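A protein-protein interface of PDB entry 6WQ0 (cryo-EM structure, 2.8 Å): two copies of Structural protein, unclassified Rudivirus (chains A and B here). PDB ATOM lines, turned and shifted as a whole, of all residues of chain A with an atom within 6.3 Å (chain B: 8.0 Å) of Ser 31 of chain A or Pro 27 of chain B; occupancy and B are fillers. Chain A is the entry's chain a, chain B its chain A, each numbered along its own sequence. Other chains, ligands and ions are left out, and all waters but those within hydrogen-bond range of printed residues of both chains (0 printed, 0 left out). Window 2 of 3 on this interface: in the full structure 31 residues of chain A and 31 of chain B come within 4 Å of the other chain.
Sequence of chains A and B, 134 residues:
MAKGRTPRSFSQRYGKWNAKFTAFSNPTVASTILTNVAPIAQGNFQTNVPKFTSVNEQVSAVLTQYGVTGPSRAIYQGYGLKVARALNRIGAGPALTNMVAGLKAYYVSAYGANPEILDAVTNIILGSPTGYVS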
ATOM      1  N   PHE A  24      22.182   7.216  25.181  1.00  0.00           N
ATOM      2  CA  PHE A  24      21.716   5.892  24.787  1.00  0.00           C
ATOM      3  C   PHE A  24      21.713   5.689  23.275  1.00  0.00           C
ATOM      4  O   PHE A  24      21.677   4.545  22.821  1.00  0.00           O
ATOM      5  CB  PHE A  24      20.318   5.644  25.354  1.00  0.00           C
ATOM      6  CG  PHE A  24      19.891   4.207  25.316  1.00  0.00           C
ATOM      7  CD1 PHE A  24      20.577   3.247  26.033  1.00  0.00           C
ATOM      8  CD2 PHE A  24      18.798   3.816  24.569  1.00  0.00           C
ATOM      9  CE1 PHE A  24      20.187   1.931  25.995  1.00  0.00           C
ATOM     10  CE2 PHE A  24      18.411   2.502  24.524  1.00  0.00           C
ATOM     11  CZ  PHE A  24      19.101   1.561  25.241  1.00  0.00           C
ATOM     12  N   ASN A  26      24.149   6.183  21.316  1.00  0.00           N
ATOM     13  CA  ASN A  26      25.444   5.673  20.896  1.00  0.00           C
ATOM     14  C   ASN A  26      25.314   4.198  20.523  1.00  0.00           C
ATOM     15  O   ASN A  26      24.552   3.466  21.160  1.00  0.00           O
ATOM     16  CB  ASN A  26      26.457   5.850  22.030  1.00  0.00           C
ATOM     17  CG  ASN A  26      27.886   5.950  21.544  1.00  0.00           C
ATOM     18  OD1 ASN A  26      28.570   4.946  21.382  1.00  0.00           O
ATOM     19  ND2 ASN A  26      28.351   7.170  21.336  1.00  0.00           N
ATOM     20  N   PRO A  27      26.019   3.731  19.490  1.00  0.00           N
ATOM     21  CA  PRO A  27      25.940   2.299  19.158  1.00  0.00           C
ATOM     22  C   PRO A  27      26.437   1.408  20.279  1.00  0.00           C
ATOM     23  O   PRO A  27      25.767   0.433  20.651  1.00  0.00           O
ATOM     24  CB  PRO A  27      26.814   2.191  17.902  1.00  0.00           C
ATOM     25  CG  PRO A  27      26.891   3.560  17.369  1.00  0.00           C
ATOM     26  CD  PRO A  27      26.858   4.467  18.535  1.00  0.00           C
ATOM     27  N   THR A  28      27.600   1.739  20.842  1.00  0.00           N
ATOM     28  CA  THR A  28      28.202   0.910  21.876  1.00  0.00           C
ATOM     29  C   THR A  28      27.366   0.908  23.146  1.00  0.00           C
ATOM     30  O   THR A  28      27.138  -0.149  23.735  1.00  0.00           O
ATOM     31  CB  THR A  28      29.621   1.391  22.166  1.00  0.00           C
ATOM     32  OG1 THR A  28      30.406   1.300  20.973  1.00  0.00           O
ATOM     33  CG2 THR A  28      30.269   0.547  23.248  1.00  0.00           C
ATOM     34  N   VAL A  29      26.887   2.074  23.577  1.00  0.00           N
ATOM     35  CA  VAL A  29      26.136   2.160  24.829  1.00  0.00           C
ATOM     36  C   VAL A  29      24.861   1.330  24.738  1.00  0.00           C
ATOM     37  O   VAL A  29      24.578   0.487  25.600  1.00  0.00           O
ATOM     38  CB  VAL A  29      25.840   3.629  25.178  1.00  0.00           C
ATOM     39  CG1 VAL A  29      25.033   3.731  26.458  1.00  0.00           C
ATOM     40  CG2 VAL A  29      27.134   4.399  25.314  1.00  0.00           C
ATOM     41  N   ALA A  30      24.087   1.545  23.673  1.00  0.00           N
ATOM     42  CA  ALA A  30      22.826   0.830  23.493  1.00  0.00           C
ATOM     43  C   ALA A  30      23.050  -0.668  23.356  1.00  0.00           C
ATOM     44  O   ALA A  30      22.388  -1.470  24.028  1.00  0.00           O
ATOM     45  CB  ALA A  30      22.091   1.375  22.273  1.00  0.00           C
ATOM     46  N   SER A  31      23.977  -1.068  22.482  1.00  0.00           N
ATOM     47  CA  SER A  31      24.210  -2.490  22.266  1.00  0.00           C
ATOM     48  C   SER A  31      24.699  -3.167  23.540  1.00  0.00           C
ATOM     49  O   SER A  31      24.264  -4.273  23.865  1.00  0.00           O
ATOM     50  CB  SER A  31      25.197  -2.698  21.121  1.00  0.00           C
ATOM     51  OG  SER A  31      26.478  -2.201  21.446  1.00  0.00           O
ATOM     52  N   THR A  32      25.586  -2.508  24.291  1.00  0.00           N
ATOM     53  CA  THR A  32      26.112  -3.094  25.518  1.00  0.00           C
ATOM     54  C   THR A  32      25.018  -3.275  26.560  1.00  0.00           C
ATOM     55  O   THR A  32      24.881  -4.352  27.150  1.00  0.00           O
ATOM     56  CB  THR A  32      27.242  -2.221  26.066  1.00  0.00           C
ATOM     57  OG1 THR A  32      28.195  -1.971  25.030  1.00  0.00           O
ATOM     58  CG2 THR A  32      27.946  -2.897  27.226  1.00  0.00           C
ATOM     59  N   ILE A  33      24.211  -2.237  26.789  1.00  0.00           N
ATOM     60  CA  ILE A  33      23.183  -2.328  27.823  1.00  0.00           C
ATOM     61  C   ILE A  33      22.149  -3.387  27.456  1.00  0.00           C
ATOM     62  O   ILE A  33      21.748  -4.206  28.294  1.00  0.00           O
ATOM     63  CB  ILE A  33      22.537  -0.952  28.064  1.00  0.00           C
ATOM     64  CG1 ILE A  33      23.564   0.027  28.635  1.00  0.00           C
ATOM     65  CG2 ILE A  33      21.355  -1.071  29.000  1.00  0.00           C
ATOM     66  CD1 ILE A  33      22.967   1.303  29.153  1.00  0.00           C
ATOM     67  N   LEU A  34      21.734  -3.419  26.186  1.00  0.00           N
ATOM     68  CA  LEU A  34      20.691  -4.360  25.793  1.00  0.00           C
ATOM     69  C   LEU A  34      21.208  -5.792  25.765  1.00  0.00           C
ATOM     70  O   LEU A  34      20.504  -6.720  26.184  1.00  0.00           O
ATOM     71  CB  LEU A  34      20.115  -3.958  24.441  1.00  0.00           C
ATOM     72  CG  LEU A  34      19.367  -2.622  24.447  1.00  0.00           C
ATOM     73  CD1 LEU A  34      18.971  -2.219  23.043  1.00  0.00           C
ATOM     74  CD2 LEU A  34      18.156  -2.670  25.357  1.00  0.00           C
ATOM     75  N   THR A  35      22.445  -5.995  25.309  1.00  0.00           N
ATOM     76  CA  THR A  35      23.013  -7.334  25.283  1.00  0.00           C
ATOM     77  C   THR A  35      23.282  -7.847  26.691  1.00  0.00           C
ATOM     78  O   THR A  35      23.240  -9.056  26.939  1.00  0.00           O
ATOM     79  CB  THR A  35      24.286  -7.323  24.438  1.00  0.00           C
ATOM     80  OG1 THR A  35      23.953  -6.968  23.093  1.00  0.00           O
ATOM     81  CG2 THR A  35      24.948  -8.679  24.426  1.00  0.00           C
ATOM     82  N   ASN A  36      23.537  -6.942  27.638  1.00  0.00           N
ATOM     83  CA  ASN A  36      23.722  -7.378  29.016  1.00  0.00           C
ATOM     84  C   ASN A  36      22.396  -7.711  29.685  1.00  0.00           C
ATOM     85  O   ASN A  36      22.325  -8.656  30.477  1.00  0.00           O
ATOM     86  CB  ASN A  36      24.474  -6.314  29.811  1.00  0.00           C
ATOM     87  CG  ASN A  36      25.932  -6.654  30.005  1.00  0.00           C
ATOM     88  OD1 ASN A  36      26.287  -7.416  30.897  1.00  0.00           O
ATOM     89  ND2 ASN A  36      26.786  -6.088  29.175  1.00  0.00           N
ATOM     90  N   THR B  22      16.012  -9.213  20.221  1.00  0.00           N
ATOM     91  CA  THR B  22      17.332  -9.617  19.756  1.00  0.00           C
ATOM     92  C   THR B  22      17.786  -8.767  18.578  1.00  0.00           C
ATOM     93  O   THR B  22      18.974  -8.450  18.454  1.00  0.00           O
ATOM     94  CB  THR B  22      17.314 -11.093  19.373  1.00  0.00           C
ATOM     95  OG1 THR B  22      16.891 -11.869  20.498  1.00  0.00           O
ATOM     96  CG2 THR B  22      18.690 -11.553  18.953  1.00  0.00           C
ATOM     97  N   ALA B  23      16.856  -8.390  17.700  1.00  0.00           N
ATOM     98  CA  ALA B  23      17.203  -7.514  16.589  1.00  0.00           C
ATOM     99  C   ALA B  23      17.601  -6.129  17.082  1.00  0.00           C
ATOM    100  O   ALA B  23      18.593  -5.559  16.619  1.00  0.00           O
ATOM    101  CB  ALA B  23      16.036  -7.419  15.609  1.00  0.00           C
ATOM    102  N   PHE B  24      16.841  -5.572  18.025  1.00  0.00           N
ATOM    103  CA  PHE B  24      17.119  -4.222  18.506  1.00  0.00           C
ATOM    104  C   PHE B  24      18.402  -4.131  19.323  1.00  0.00           C
ATOM    105  O   PHE B  24      18.906  -3.027  19.529  1.00  0.00           O
ATOM    106  CB  PHE B  24      15.936  -3.707  19.329  1.00  0.00           C
ATOM    107  CG  PHE B  24      16.004  -2.240  19.642  1.00  0.00           C
ATOM    108  CD1 PHE B  24      15.939  -1.298  18.631  1.00  0.00           C
ATOM    109  CD2 PHE B  24      16.126  -1.802  20.949  1.00  0.00           C
ATOM    110  CE1 PHE B  24      16.006   0.045  18.917  1.00  0.00           C
ATOM    111  CE2 PHE B  24      16.190  -0.459  21.239  1.00  0.00           C
ATOM    112  CZ  PHE B  24      16.132   0.464  20.223  1.00  0.00           C
ATOM    113  N   SER B  25      18.945  -5.252  19.796  1.00  0.00           N
ATOM    114  CA  SER B  25      20.210  -5.223  20.519  1.00  0.00           C
ATOM    115  C   SER B  25      21.417  -5.102  19.602  1.00  0.00           C
ATOM    116  O   SER B  25      22.533  -4.936  20.101  1.00  0.00           O
ATOM    117  CB  SER B  25      20.351  -6.468  21.389  1.00  0.00           C
ATOM    118  OG  SER B  25      19.166  -6.702  22.122  1.00  0.00           O
ATOM    119  N   ASN B  26      21.225  -5.195  18.293  1.00  0.00           N
ATOM    120  CA  ASN B  26      22.303  -4.947  17.350  1.00  0.00           C
ATOM    121  C   ASN B  26      22.776  -3.502  17.489  1.00  0.00           C
ATOM    122  O   ASN B  26      21.960  -2.604  17.715  1.00  0.00           O
ATOM    123  CB  ASN B  26      21.812  -5.212  15.924  1.00  0.00           C
ATOM    124  CG  ASN B  26      22.923  -5.603  14.974  1.00  0.00           C
ATOM    125  OD1 ASN B  26      23.529  -4.756  14.325  1.00  0.00           O
ATOM    126  ND2 ASN B  26      23.172  -6.896  14.863  1.00  0.00           N
ATOM    127  N   PRO B  27      24.080  -3.238  17.372  1.00  0.00           N
ATOM    128  CA  PRO B  27      24.538  -1.842  17.473  1.00  0.00           C
ATOM    129  C   PRO B  27      23.984  -0.953  16.374  1.00  0.00           C
ATOM    130  O   PRO B  27      23.502   0.153  16.650  1.00  0.00           O
ATOM    131  CB  PRO B  27      26.064  -1.976  17.393  1.00  0.00           C
ATOM    132  CG  PRO B  27      26.350  -3.380  17.744  1.00  0.00           C
ATOM    133  CD  PRO B  27      25.204  -4.177  17.246  1.00  0.00           C
ATOM    134  N   THR B  28      24.027  -1.420  15.125  1.00  0.00           N
ATOM    135  CA  THR B  28      23.578  -0.599  14.008  1.00  0.00           C
ATOM    136  C   THR B  28      22.071  -0.390  14.037  1.00  0.00           C
ATOM    137  O   THR B  28      21.595   0.719  13.787  1.00  0.00           O
ATOM    138  CB  THR B  28      24.009  -1.234  12.689  1.00  0.00           C
ATOM    139  OG1 THR B  28      25.438  -1.314  12.644  1.00  0.00           O
ATOM    140  CG2 THR B  28      23.521  -0.409  11.510  1.00  0.00           C
ATOM    141  N   VAL B  29      21.304  -1.431  14.359  1.00  0.00           N
ATOM    142  CA  VAL B  29      19.848  -1.306  14.374  1.00  0.00           C
ATOM    143  C   VAL B  29      19.414  -0.265  15.399  1.00  0.00           C
ATOM    144  O   VAL B  29      18.730   0.713  15.072  1.00  0.00           O
ATOM    145  CB  VAL B  29      19.193  -2.673  14.640  1.00  0.00           C
ATOM    146  CG1 VAL B  29      17.700  -2.520  14.817  1.00  0.00           C
ATOM    147  CG2 VAL B  29      19.491  -3.626  13.502  1.00  0.00           C
ATOM    148  N   ALA B  30      19.811  -0.464  16.656  1.00  0.00           N
ATOM    149  CA  ALA B  30      19.428   0.455  17.723  1.00  0.00           C
ATOM    150  C   ALA B  30      19.951   1.857  17.455  1.00  0.00           C
ATOM    151  O   ALA B  30      19.224   2.845  17.614  1.00  0.00           O
ATOM    152  CB  ALA B  30      19.946  -0.063  19.063  1.00  0.00           C
ATOM    153  N   SER B  31      21.216   1.960  17.047  1.00  0.00           N
ATOM    154  CA  SER B  31      21.820   3.260  16.788  1.00  0.00           C
ATOM    155  C   SER B  31      21.061   4.019  15.708  1.00  0.00           C
ATOM    156  O   SER B  31      20.715   5.189  15.888  1.00  0.00           O
ATOM    157  CB  SER B  31      23.281   3.070  16.393  1.00  0.00           C
ATOM    158  OG  SER B  31      23.785   4.206  15.724  1.00  0.00           O
ATOM    159  N   THR B  32      20.788   3.366  14.576  1.00  0.00           N
ATOM    160  CA  THR B  32      20.093   4.020  13.476  1.00  0.00           C
ATOM    161  C   THR B  32      18.690   4.445  13.883  1.00  0.00           C
ATOM    162  O   THR B  32      18.275   5.578  13.619  1.00  0.00           O
ATOM    163  CB  THR B  32      20.043   3.085  12.267  1.00  0.00           C
ATOM    164  OG1 THR B  32      21.355   2.584  12.000  1.00  0.00           O
ATOM    165  CG2 THR B  32      19.538   3.813  11.044  1.00  0.00           C
ATOM    166  N   ILE B  33      17.949   3.556  14.548  1.00  0.00           N
ATOM    167  CA  ILE B  33      16.570   3.878  14.910  1.00  0.00           C
ATOM    168  C   ILE B  33      16.529   5.061  15.868  1.00  0.00           C
ATOM    169  O   ILE B  33      15.774   6.020  15.667  1.00  0.00           O
ATOM    170  CB  ILE B  33      15.863   2.645  15.500  1.00  0.00           C
ATOM    171  CG1 ILE B  33      15.772   1.531  14.461  1.00  0.00           C
ATOM    172  CG2 ILE B  33      14.474   3.003  15.981  1.00  0.00           C
ATOM    173  CD1 ILE B  33      14.992   0.339  14.928  1.00  0.00           C
ATOM    174  N   LEU B  34      17.349   5.020  16.920  1.00  0.00           N
ATOM    175  CA  LEU B  34      17.296   6.074  17.925  1.00  0.00           C
ATOM    176  C   LEU B  34      17.828   7.394  17.383  1.00  0.00           C
ATOM    177  O   LEU B  34      17.266   8.457  17.667  1.00  0.00           O
ATOM    178  CB  LEU B  34      18.063   5.640  19.172  1.00  0.00           C
ATOM    179  CG  LEU B  34      17.494   4.409  19.879  1.00  0.00           C
ATOM    180  CD1 LEU B  34      18.345   4.019  21.063  1.00  0.00           C
ATOM    181  CD2 LEU B  34      16.059   4.645  20.300  1.00  0.00           C
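Phe 24 of chain A touches Leu 34 of chain B, and with the chains exchanged Leu 34 of chain A touches Phe 24 of chain B. Pro 27 of chain A touches Ser 31 of chain B, and with the chains exchanged Ser 31 of chain A touches Pro 27 of chain B. Positions printed for both chains: 24, 26, 27, 28, 29, 30, 31, 32, 33 and 34. Of the 7 pairs that touch across the chains among the printed residues, 4 have their exchanged pair printed and touching as well.
Of the printed residues of chain B, Leu 34 of chain A touches Phe 24 (3.6 Å) and Ser 25 (3.7 Å). Printed residues of chain B within 4 Å of Thr 35 of chain A: Ser 25 (3.9 Å). Of the printed residues of chain A, Ser 25 of chain B touches Ser 31, Leu 34 and Thr 35. Printed residues of chain A within 4 Å of Pro 27 of chain B: Ser 31 (3.6 Å). The nearest residue of chain B that does not touch Ser 31 of chain A is Asn 26 of chain B (4.4 Å).
Phe 24 of chain A touches Leu 34 of chain B (CD2 to CD1, 3.5 Å). Pro 27 of chain A touches Ser 31 of chain B. CB of Ser 31 of chain A touches O of Ser 25 of chain B, 3.6 Å away. CB of Ser 31 of chain A touches CG of Pro 27 of chain B, at 3.6 Å. Phe 24 of chain B touches Leu 34 of chain A (CD2 to CD1, 3.6 Å). OG of Ser 25 of chain B touches CB of Leu 34 of chain A (3.7 Å). OG1 of Thr 35 of chain A touches O of Ser 25 of chain B, at 3.9 Å.
Printed residues of chain B that touch a printed residue of chain A: Phe 24, Ser 25, Pro 27, Ser 31 and Leu 34. Hydrophobic or aromatic side chains of chain B within 4 Å of the printed part of chain A: Phe 24, Pro 27 and Leu 34. Printed residues of chain A that touch a printed residue of chain B: Phe 24, Pro 27, Ser 31, Leu 34 and Thr 35. Hydrophobic or aromatic side chains of chain A within 4 Å of the printed part of chain B: Phe 24, Pro 27 and Leu 34. Among the printed residues, 7 pairs touch across the chains. Among the printed residues, no Asp or Glu carboxylate lies within 4 Å of a Lys or Arg side-chain nitrogen of the other chain.
O of Pro 27 of chain A sits at hydrogen-bond distance from OG of Ser 31 of chain A, at 2.8 Å. The side-chain hydroxyl (OG) of Ser 31 of chain A sits at hydrogen-bond distance from the backbone carbonyl oxygen (O) of Thr 28 of chain A. The side-chain hydroxyl (OG1) of Thr 35 of chain A is in hydrogen-bond range of the backbone carbonyl oxygen (O) of Ser 31 of chain A, at 2.8 Å.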
